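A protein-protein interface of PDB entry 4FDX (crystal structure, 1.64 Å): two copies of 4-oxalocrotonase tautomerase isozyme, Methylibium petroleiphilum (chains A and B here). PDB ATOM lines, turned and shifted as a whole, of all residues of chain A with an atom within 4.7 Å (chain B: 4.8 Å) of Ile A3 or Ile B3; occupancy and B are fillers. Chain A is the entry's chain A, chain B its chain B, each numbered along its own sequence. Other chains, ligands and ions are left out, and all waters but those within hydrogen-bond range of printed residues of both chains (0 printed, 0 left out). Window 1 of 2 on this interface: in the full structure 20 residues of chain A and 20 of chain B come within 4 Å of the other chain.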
ATOM      1  N   PRO A   1       5.281  22.815  37.366  1.00  0.00           N
ATOM      2  CA  PRO A   1       4.643  22.231  36.163  1.00  0.00           C
ATOM      3  C   PRO A   1       5.501  22.468  34.959  1.00  0.00           C
ATOM      4  O   PRO A   1       6.058  23.551  34.753  1.00  0.00           O
ATOM      5  CB  PRO A   1       3.274  22.947  36.090  1.00  0.00           C
ATOM      6  CG  PRO A   1       3.022  23.316  37.547  1.00  0.00           C
ATOM      7  CD  PRO A   1       4.329  23.598  38.191  1.00  0.00           C
ATOM      8  N   ILE A   2       5.532  21.501  34.063  1.00  0.00           N
ATOM      9  CA  ILE A   2       6.288  21.590  32.836  1.00  0.00           C
ATOM     10  C   ILE A   2       5.226  21.411  31.744  1.00  0.00           C
ATOM     11  O   ILE A   2       4.478  20.398  31.733  1.00  0.00           O
ATOM     12  CB  ILE A   2       7.376  20.518  32.763  1.00  0.00           C
ATOM     13  CG1 ILE A   2       8.484  20.889  33.800  1.00  0.00           C
ATOM     14  CG2 ILE A   2       8.010  20.518  31.369  1.00  0.00           C
ATOM     15  CD1 ILE A   2       9.548  19.811  33.987  1.00  0.00           C
ATOM     16  N   ILE A   3       5.108  22.399  30.853  1.00  0.00           N
ATOM     17  CA  ILE A   3       4.022  22.386  29.836  1.00  0.00           C
ATOM     18  C   ILE A   3       4.679  22.319  28.484  1.00  0.00           C
ATOM     19  O   ILE A   3       5.624  23.028  28.215  1.00  0.00           O
ATOM     20  CB  ILE A   3       3.245  23.633  29.957  1.00  0.00           C
ATOM     21  CG1 ILE A   3       2.523  23.476  31.295  1.00  0.00           C
ATOM     22  CG2 ILE A   3       2.286  23.788  28.756  1.00  0.00           C
ATOM     23  CD1 ILE A   3       2.043  24.788  31.678  1.00  0.00           C
ATOM     24  N   GLN A   4       4.251  21.387  27.624  1.00  0.00           N
ATOM     25  CA  GLN A   4       4.755  21.321  26.258  1.00  0.00           C
ATOM     26  C   GLN A   4       3.615  21.746  25.384  1.00  0.00           C
ATOM     27  O   GLN A   4       2.530  21.169  25.526  1.00  0.00           O
ATOM     28  CB  GLN A   4       5.160  19.859  25.929  1.00  0.00           C
ATOM     29  CG  GLN A   4       6.378  19.497  26.732  1.00  0.00           C
ATOM     30  CD  GLN A   4       6.600  17.977  26.912  1.00  0.00           C
ATOM     31  OE1 GLN A   4       5.862  17.249  27.634  1.00  0.00           O
ATOM     32  NE2 GLN A   4       7.654  17.504  26.264  1.00  0.00           N
ATOM     33  N   MET A   5       3.826  22.721  24.542  1.00  0.00           N
ATOM     34  CA  MET A   5       2.736  23.147  23.696  1.00  0.00           C
ATOM     35  C   MET A   5       3.128  22.875  22.235  1.00  0.00           C
ATOM     36  O   MET A   5       4.116  23.432  21.710  1.00  0.00           O
ATOM     37  CB  MET A   5       2.547  24.592  23.899  1.00  0.00           C
ATOM     38  CG  MET A   5       1.485  25.132  22.945  1.00  0.00           C
ATOM     39  SD  MET A   5       0.649  26.655  23.352  1.00  0.00           S
ATOM     40  CE  MET A   5       1.918  27.769  23.374  1.00  0.00           C
ATOM     41  N   ILE A  23      -0.363  31.607  29.606  1.00  0.00           N
ATOM     42  CA  ILE A  23      -0.488  30.238  30.144  1.00  0.00           C
ATOM     43  C   ILE A  23       0.200  30.167  31.535  1.00  0.00           C
ATOM     44  O   ILE A  23      -0.342  29.499  32.479  1.00  0.00           O
ATOM     45  CB  ILE A  23       0.198  29.221  29.177  1.00  0.00           C
ATOM     46  CG1 ILE A  23      -0.666  29.078  27.915  1.00  0.00           C
ATOM     47  CG2 ILE A  23       0.441  27.890  29.902  1.00  0.00           C
ATOM     48  CD1 ILE A  23       0.119  28.419  26.763  1.00  0.00           C
ATOM     49  N   VAL A  27      -1.533  29.031  35.176  1.00  0.00           N
ATOM     50  CA  VAL A  27      -0.996  27.879  35.986  1.00  0.00           C
ATOM     51  C   VAL A  27      -0.712  28.422  37.369  1.00  0.00           C
ATOM     52  O   VAL A  27      -1.125  27.855  38.338  1.00  0.00           O
ATOM     53  CB  VAL A  27       0.251  27.317  35.288  1.00  0.00           C
ATOM     54  CG1 VAL A  27       0.846  26.234  36.203  1.00  0.00           C
ATOM     55  CG2 VAL A  27      -0.213  26.635  33.970  1.00  0.00           C
ATOM     56  N   VAL A  38       7.045  27.241  36.748  1.00  0.00           N
ATOM     57  CA  VAL A  38       6.310  26.914  35.486  1.00  0.00           C
ATOM     58  C   VAL A  38       7.223  27.059  34.282  1.00  0.00           C
ATOM     59  O   VAL A  38       7.769  28.165  34.012  1.00  0.00           O
ATOM     60  CB  VAL A  38       5.091  27.894  35.341  1.00  0.00           C
ATOM     61  CG1 VAL A  38       4.327  27.612  34.028  1.00  0.00           C
ATOM     62  CG2 VAL A  38       4.233  27.768  36.621  1.00  0.00           C
ATOM     63  N   ARG A  39       7.434  25.949  33.599  1.00  0.00           N
ATOM     64  CA  ARG A  39       8.276  25.977  32.405  1.00  0.00           C
ATOM     65  C   ARG A  39       7.424  25.582  31.214  1.00  0.00           C
ATOM     66  O   ARG A  39       6.592  24.711  31.294  1.00  0.00           O
ATOM     67  CB  ARG A  39       9.412  25.007  32.572  1.00  0.00           C
ATOM     68  CG  ARG A  39      10.516  25.603  33.444  1.00  0.00           C
ATOM     69  CD  ARG A  39      11.487  24.524  33.940  1.00  0.00           C
ATOM     70  NE  ARG A  39      12.602  25.250  34.565  1.00  0.00           N
ATOM     71  CZ  ARG A  39      12.456  25.836  35.748  1.00  0.00           C
ATOM     72  NH1 ARG A  39      11.349  25.678  36.458  1.00  0.00           N
ATOM     73  NH2 ARG A  39      13.431  26.573  36.256  1.00  0.00           N
ATOM     74  N   ILE A  40       7.536  26.353  30.148  1.00  0.00           N
ATOM     75  CA  ILE A  40       6.791  26.015  28.909  1.00  0.00           C
ATOM     76  C   ILE A  40       7.785  25.765  27.751  1.00  0.00           C
ATOM     77  O   ILE A  40       8.780  26.546  27.546  1.00  0.00           O
ATOM     78  CB  ILE A  40       5.850  27.093  28.492  1.00  0.00           C
ATOM     79  CG1 ILE A  40       4.835  27.440  29.621  1.00  0.00           C
ATOM     80  CG2 ILE A  40       5.063  26.657  27.200  1.00  0.00           C
ATOM     81  CD1 ILE A  40       4.071  28.734  29.391  1.00  0.00           C
ATOM     82  N   LEU A  41       7.557  24.666  27.052  1.00  0.00           N
ATOM     83  CA  LEU A  41       8.396  24.295  25.881  1.00  0.00           C
ATOM     84  C   LEU A  41       7.441  24.407  24.666  1.00  0.00           C
ATOM     85  O   LEU A  41       6.368  23.782  24.679  1.00  0.00           O
ATOM     86  CB  LEU A  41       8.902  22.891  26.075  1.00  0.00           C
ATOM     87  CG  LEU A  41       9.991  22.643  27.122  1.00  0.00           C
ATOM     88  CD1 LEU A  41       9.486  23.033  28.507  1.00  0.00           C
ATOM     89  CD2 LEU A  41      10.306  21.156  27.100  1.00  0.00           C
ATOM     90  N   PRO B   1      -3.986  23.626  18.952  1.00  0.00           N
ATOM     91  CA  PRO B   1      -2.824  23.394  19.808  1.00  0.00           C
ATOM     92  C   PRO B   1      -3.044  22.186  20.685  1.00  0.00           C
ATOM     93  O   PRO B   1      -4.137  21.983  21.185  1.00  0.00           O
ATOM     94  CB  PRO B   1      -2.682  24.746  20.572  1.00  0.00           C
ATOM     95  CG  PRO B   1      -3.183  25.742  19.539  1.00  0.00           C
ATOM     96  CD  PRO B   1      -4.331  25.063  18.879  1.00  0.00           C
ATOM     97  N   ILE B   2      -2.001  21.413  20.870  1.00  0.00           N
ATOM     98  CA  ILE B   2      -2.070  20.260  21.844  1.00  0.00           C
ATOM     99  C   ILE B   2      -1.085  20.494  22.969  1.00  0.00           C
ATOM    100  O   ILE B   2       0.142  20.677  22.682  1.00  0.00           O
ATOM    101  CB  ILE B   2      -1.695  18.991  21.130  1.00  0.00           C
ATOM    102  CG1 ILE B   2      -2.834  18.721  20.120  1.00  0.00           C
ATOM    103  CG2 ILE B   2      -1.550  17.828  22.128  1.00  0.00           C
ATOM    104  CD1 ILE B   2      -2.544  17.719  19.015  1.00  0.00           C
ATOM    105  N   ILE B   3      -1.573  20.508  24.215  1.00  0.00           N
ATOM    106  CA  ILE B   3      -0.753  20.935  25.380  1.00  0.00           C
ATOM    107  C   ILE B   3      -0.588  19.701  26.260  1.00  0.00           C
ATOM    108  O   ILE B   3      -1.580  19.074  26.586  1.00  0.00           O
ATOM    109  CB  ILE B   3      -1.435  22.072  26.092  1.00  0.00           C
ATOM    110  CG1 ILE B   3      -1.467  23.260  25.080  1.00  0.00           C
ATOM    111  CG2 ILE B   3      -0.719  22.318  27.446  1.00  0.00           C
ATOM    112  CD1 ILE B   3      -2.420  24.281  25.528  1.00  0.00           C
ATOM    113  N   GLN B   4       0.648  19.310  26.593  1.00  0.00           N
ATOM    114  CA  GLN B   4       0.861  18.310  27.653  1.00  0.00           C
ATOM    115  C   GLN B   4       1.341  19.004  28.929  1.00  0.00           C
ATOM    116  O   GLN B   4       2.245  19.775  28.884  1.00  0.00           O
ATOM    117  CB  GLN B   4       1.862  17.227  27.259  1.00  0.00           C
ATOM    118  CG  GLN B   4       1.351  16.426  26.063  1.00  0.00           C
ATOM    119  CD  GLN B   4       2.448  15.922  25.118  1.00  0.00           C
ATOM    120  OE1 GLN B   4       3.038  16.701  24.315  1.00  0.00           O
ATOM    121  NE2 GLN B   4       2.695  14.606  25.180  1.00  0.00           N
ATOM    122  N   MET B   5       0.636  18.787  30.025  1.00  0.00           N
ATOM    123  CA  MET B   5       1.012  19.407  31.290  1.00  0.00           C
ATOM    124  C   MET B   5       1.466  18.289  32.210  1.00  0.00           C
ATOM    125  O   MET B   5       0.709  17.415  32.556  1.00  0.00           O
ATOM    126  CB  MET B   5      -0.173  20.196  31.824  1.00  0.00           C
ATOM    127  CG  MET B   5       0.230  20.619  33.252  1.00  0.00           C
ATOM    128  SD  MET B   5      -0.817  21.972  33.850  1.00  0.00           S
ATOM    129  CE  MET B   5      -2.354  21.188  33.947  1.00  0.00           C
ATOM    130  N   ILE B  23      -6.036  27.397  31.146  1.00  0.00           N
ATOM    131  CA  ILE B  23      -5.024  27.236  30.059  1.00  0.00           C
ATOM    132  C   ILE B  23      -5.693  27.321  28.702  1.00  0.00           C
ATOM    133  O   ILE B  23      -5.186  27.952  27.763  1.00  0.00           O
ATOM    134  CB  ILE B  23      -4.194  25.909  30.229  1.00  0.00           C
ATOM    135  CG1 ILE B  23      -3.323  26.030  31.484  1.00  0.00           C
ATOM    136  CG2 ILE B  23      -3.330  25.620  28.977  1.00  0.00           C
ATOM    137  CD1 ILE B  23      -2.728  24.685  31.962  1.00  0.00           C
ATOM    138  N   VAL B  27      -4.942  30.103  25.659  1.00  0.00           N
ATOM    139  CA  VAL B  27      -4.450  29.691  24.309  1.00  0.00           C
ATOM    140  C   VAL B  27      -5.427  30.282  23.261  1.00  0.00           C
ATOM    141  O   VAL B  27      -4.979  30.885  22.287  1.00  0.00           O
ATOM    142  CB  VAL B  27      -4.380  28.158  24.258  1.00  0.00           C
ATOM    143  CG1 VAL B  27      -4.249  27.673  22.799  1.00  0.00           C
ATOM    144  CG2 VAL B  27      -3.141  27.719  25.033  1.00  0.00           C
ATOM    145  N   VAL B  38      -8.292  23.119  20.958  1.00  0.00           N
ATOM    146  CA  VAL B  38      -7.325  23.101  22.092  1.00  0.00           C
ATOM    147  C   VAL B  38      -7.505  21.850  22.934  1.00  0.00           C
ATOM    148  O   VAL B  38      -8.571  21.653  23.535  1.00  0.00           O
ATOM    149  CB  VAL B  38      -7.432  24.338  22.993  1.00  0.00           C
ATOM    150  CG1 VAL B  38      -6.319  24.333  24.042  1.00  0.00           C
ATOM    151  CG2 VAL B  38      -7.264  25.572  22.110  1.00  0.00           C
ATOM    152  N   ARG B  39      -6.483  20.984  22.900  1.00  0.00           N
ATOM    153  CA  ARG B  39      -6.540  19.760  23.732  1.00  0.00           C
ATOM    154  C   ARG B  39      -5.421  19.775  24.785  1.00  0.00           C
ATOM    155  O   ARG B  39      -4.334  20.288  24.527  1.00  0.00           O
ATOM    156  CB  ARG B  39      -6.357  18.530  22.844  1.00  0.00           C
ATOM    157  CG  ARG B  39      -7.630  18.286  22.023  1.00  0.00           C
ATOM    158  CD  ARG B  39      -7.324  17.299  20.877  1.00  0.00           C
ATOM    159  NE  ARG B  39      -8.636  16.932  20.322  1.00  0.00           N
ATOM    160  CZ  ARG B  39      -9.401  17.788  19.656  1.00  0.00           C
ATOM    161  NH1 ARG B  39      -8.996  18.988  19.293  1.00  0.00           N
ATOM    162  NH2 ARG B  39     -10.610  17.372  19.236  1.00  0.00           N
ATOM    163  N   ILE B  40      -5.759  19.411  26.026  1.00  0.00           N
ATOM    164  CA  ILE B  40      -4.747  19.329  27.053  1.00  0.00           C
ATOM    165  C   ILE B  40      -4.716  17.895  27.567  1.00  0.00           C
ATOM    166  O   ILE B  40      -5.809  17.243  27.842  1.00  0.00           O
ATOM    167  CB  ILE B  40      -5.142  20.277  28.243  1.00  0.00           C
ATOM    168  CG1 ILE B  40      -5.276  21.716  27.680  1.00  0.00           C
ATOM    169  CG2 ILE B  40      -4.009  20.180  29.285  1.00  0.00           C
ATOM    170  CD1 ILE B  40      -5.647  22.771  28.668  1.00  0.00           C
ATOM    171  N   LEU B  41      -3.490  17.401  27.763  1.00  0.00           N
ATOM    172  CA  LEU B  41      -3.271  16.047  28.311  1.00  0.00           C
ATOM    173  C   LEU B  41      -2.516  16.313  29.619  1.00  0.00           C
ATOM    174  O   LEU B  41      -1.506  17.026  29.575  1.00  0.00           O
ATOM    175  CB  LEU B  41      -2.334  15.211  27.378  1.00  0.00           C
ATOM    176  CG  LEU B  41      -2.986  14.812  26.075  1.00  0.00           C
ATOM    177  CD1 LEU B  41      -3.540  15.918  25.164  1.00  0.00           C
ATOM    178  CD2 LEU B  41      -1.957  13.981  25.362  1.00  0.00           C
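Printed residues of chain B that touch a printed residue of chain A: Ile B2, Ile B3, Gln B4, Met B5, Ile B23 and Val B27. Hydrophobic or aromatic side chains of chain B within 4 Å of the printed part of chain A: Ile B3, Ile B23 and Val B27. Among the printed residues, 10 pairs touch across the chains.
Among the printed residues, merely in contact across the chains: Ile A2 with Gln B4 (3.7 Å), Ile A2 with Met B5 (3.6 Å), Ile A3 with Ile B3 (3.6 Å), Ile A3 with Gln B4 (3.3 Å), Gln A4 with Ile B2 (3.7 Å), Gln A4 with Ile B3 (3.3 Å), Met A5 with Ile B2 (3.7 Å), Ile A23 with Val B27 (3.8 Å) and Val A27 with Ile B23 (3.8 Å).
The backbone carbonyl oxygen of Arg A39 lies within hydrogen-bond range of the backbone NH of Ile A3 (2.8 Å). The backbone carbonyl oxygen of Ile A3 lies within hydrogen-bond range of the backbone NH of Leu A41, 2.8 Å away. N of Met A5 is in hydrogen-bond range of O of Leu A41, at 2.8 Å. N of Ile B3 is in hydrogen-bond range of O of Arg B39 (2.8 Å). The backbone NH (N) of Leu B41 is in hydrogen-bond range of the backbone carbonyl oxygen (O) of Ile B3, at 2.8 Å. N of Met B5 sits at hydrogen-bond distance from O of Leu B41, at 2.8 Å.
Of chain B, only Ile B3 (3.6 Å) and Gln B4 (3.3 Å) come within 4 Å of Ile A3. Of chain A, only Ile A3 (3.6 Å) and Gln A4 (3.3 Å) come within 4 Å of Ile B3. Of the printed residues of chain A, Ile B2 touches Gln A4 and Met A5. Of the printed residues of chain B, Ile A2 touches Gln B4 and Met B5. Val B38 touches none of the printed residues of chain A. Pro B1 touches none of the printed residues of chain A. The nearest residue of chain B that does not touch Ile A3 is Met B5 (4.2 Å). The nearest residue of chain A that does not touch Ile B3 is Met A5 (4.1 Å).
The backbone carbonyl oxygen of Gln A4 lies within hydrogen-bond range of the backbone NH of Gln B4, 2.9 Å away.
Ile A2 touches Met B5, and with the chains exchanged Met A5 touches Ile B2. Ile B3 touches its own counterpart, Ile A3. Ile A3 touches Gln B4, and with the chains exchanged Gln A4 touches Ile B3. Gln B4 touches its own counterpart, Gln A4. Positions printed for both chains: 1, 2, 3, 4, 5, 23, 27, 38, 39, 40 and 41. Of the 10 pairs that touch across the chains among the printed residues, 10 have their exchanged pair printed and touching as well.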
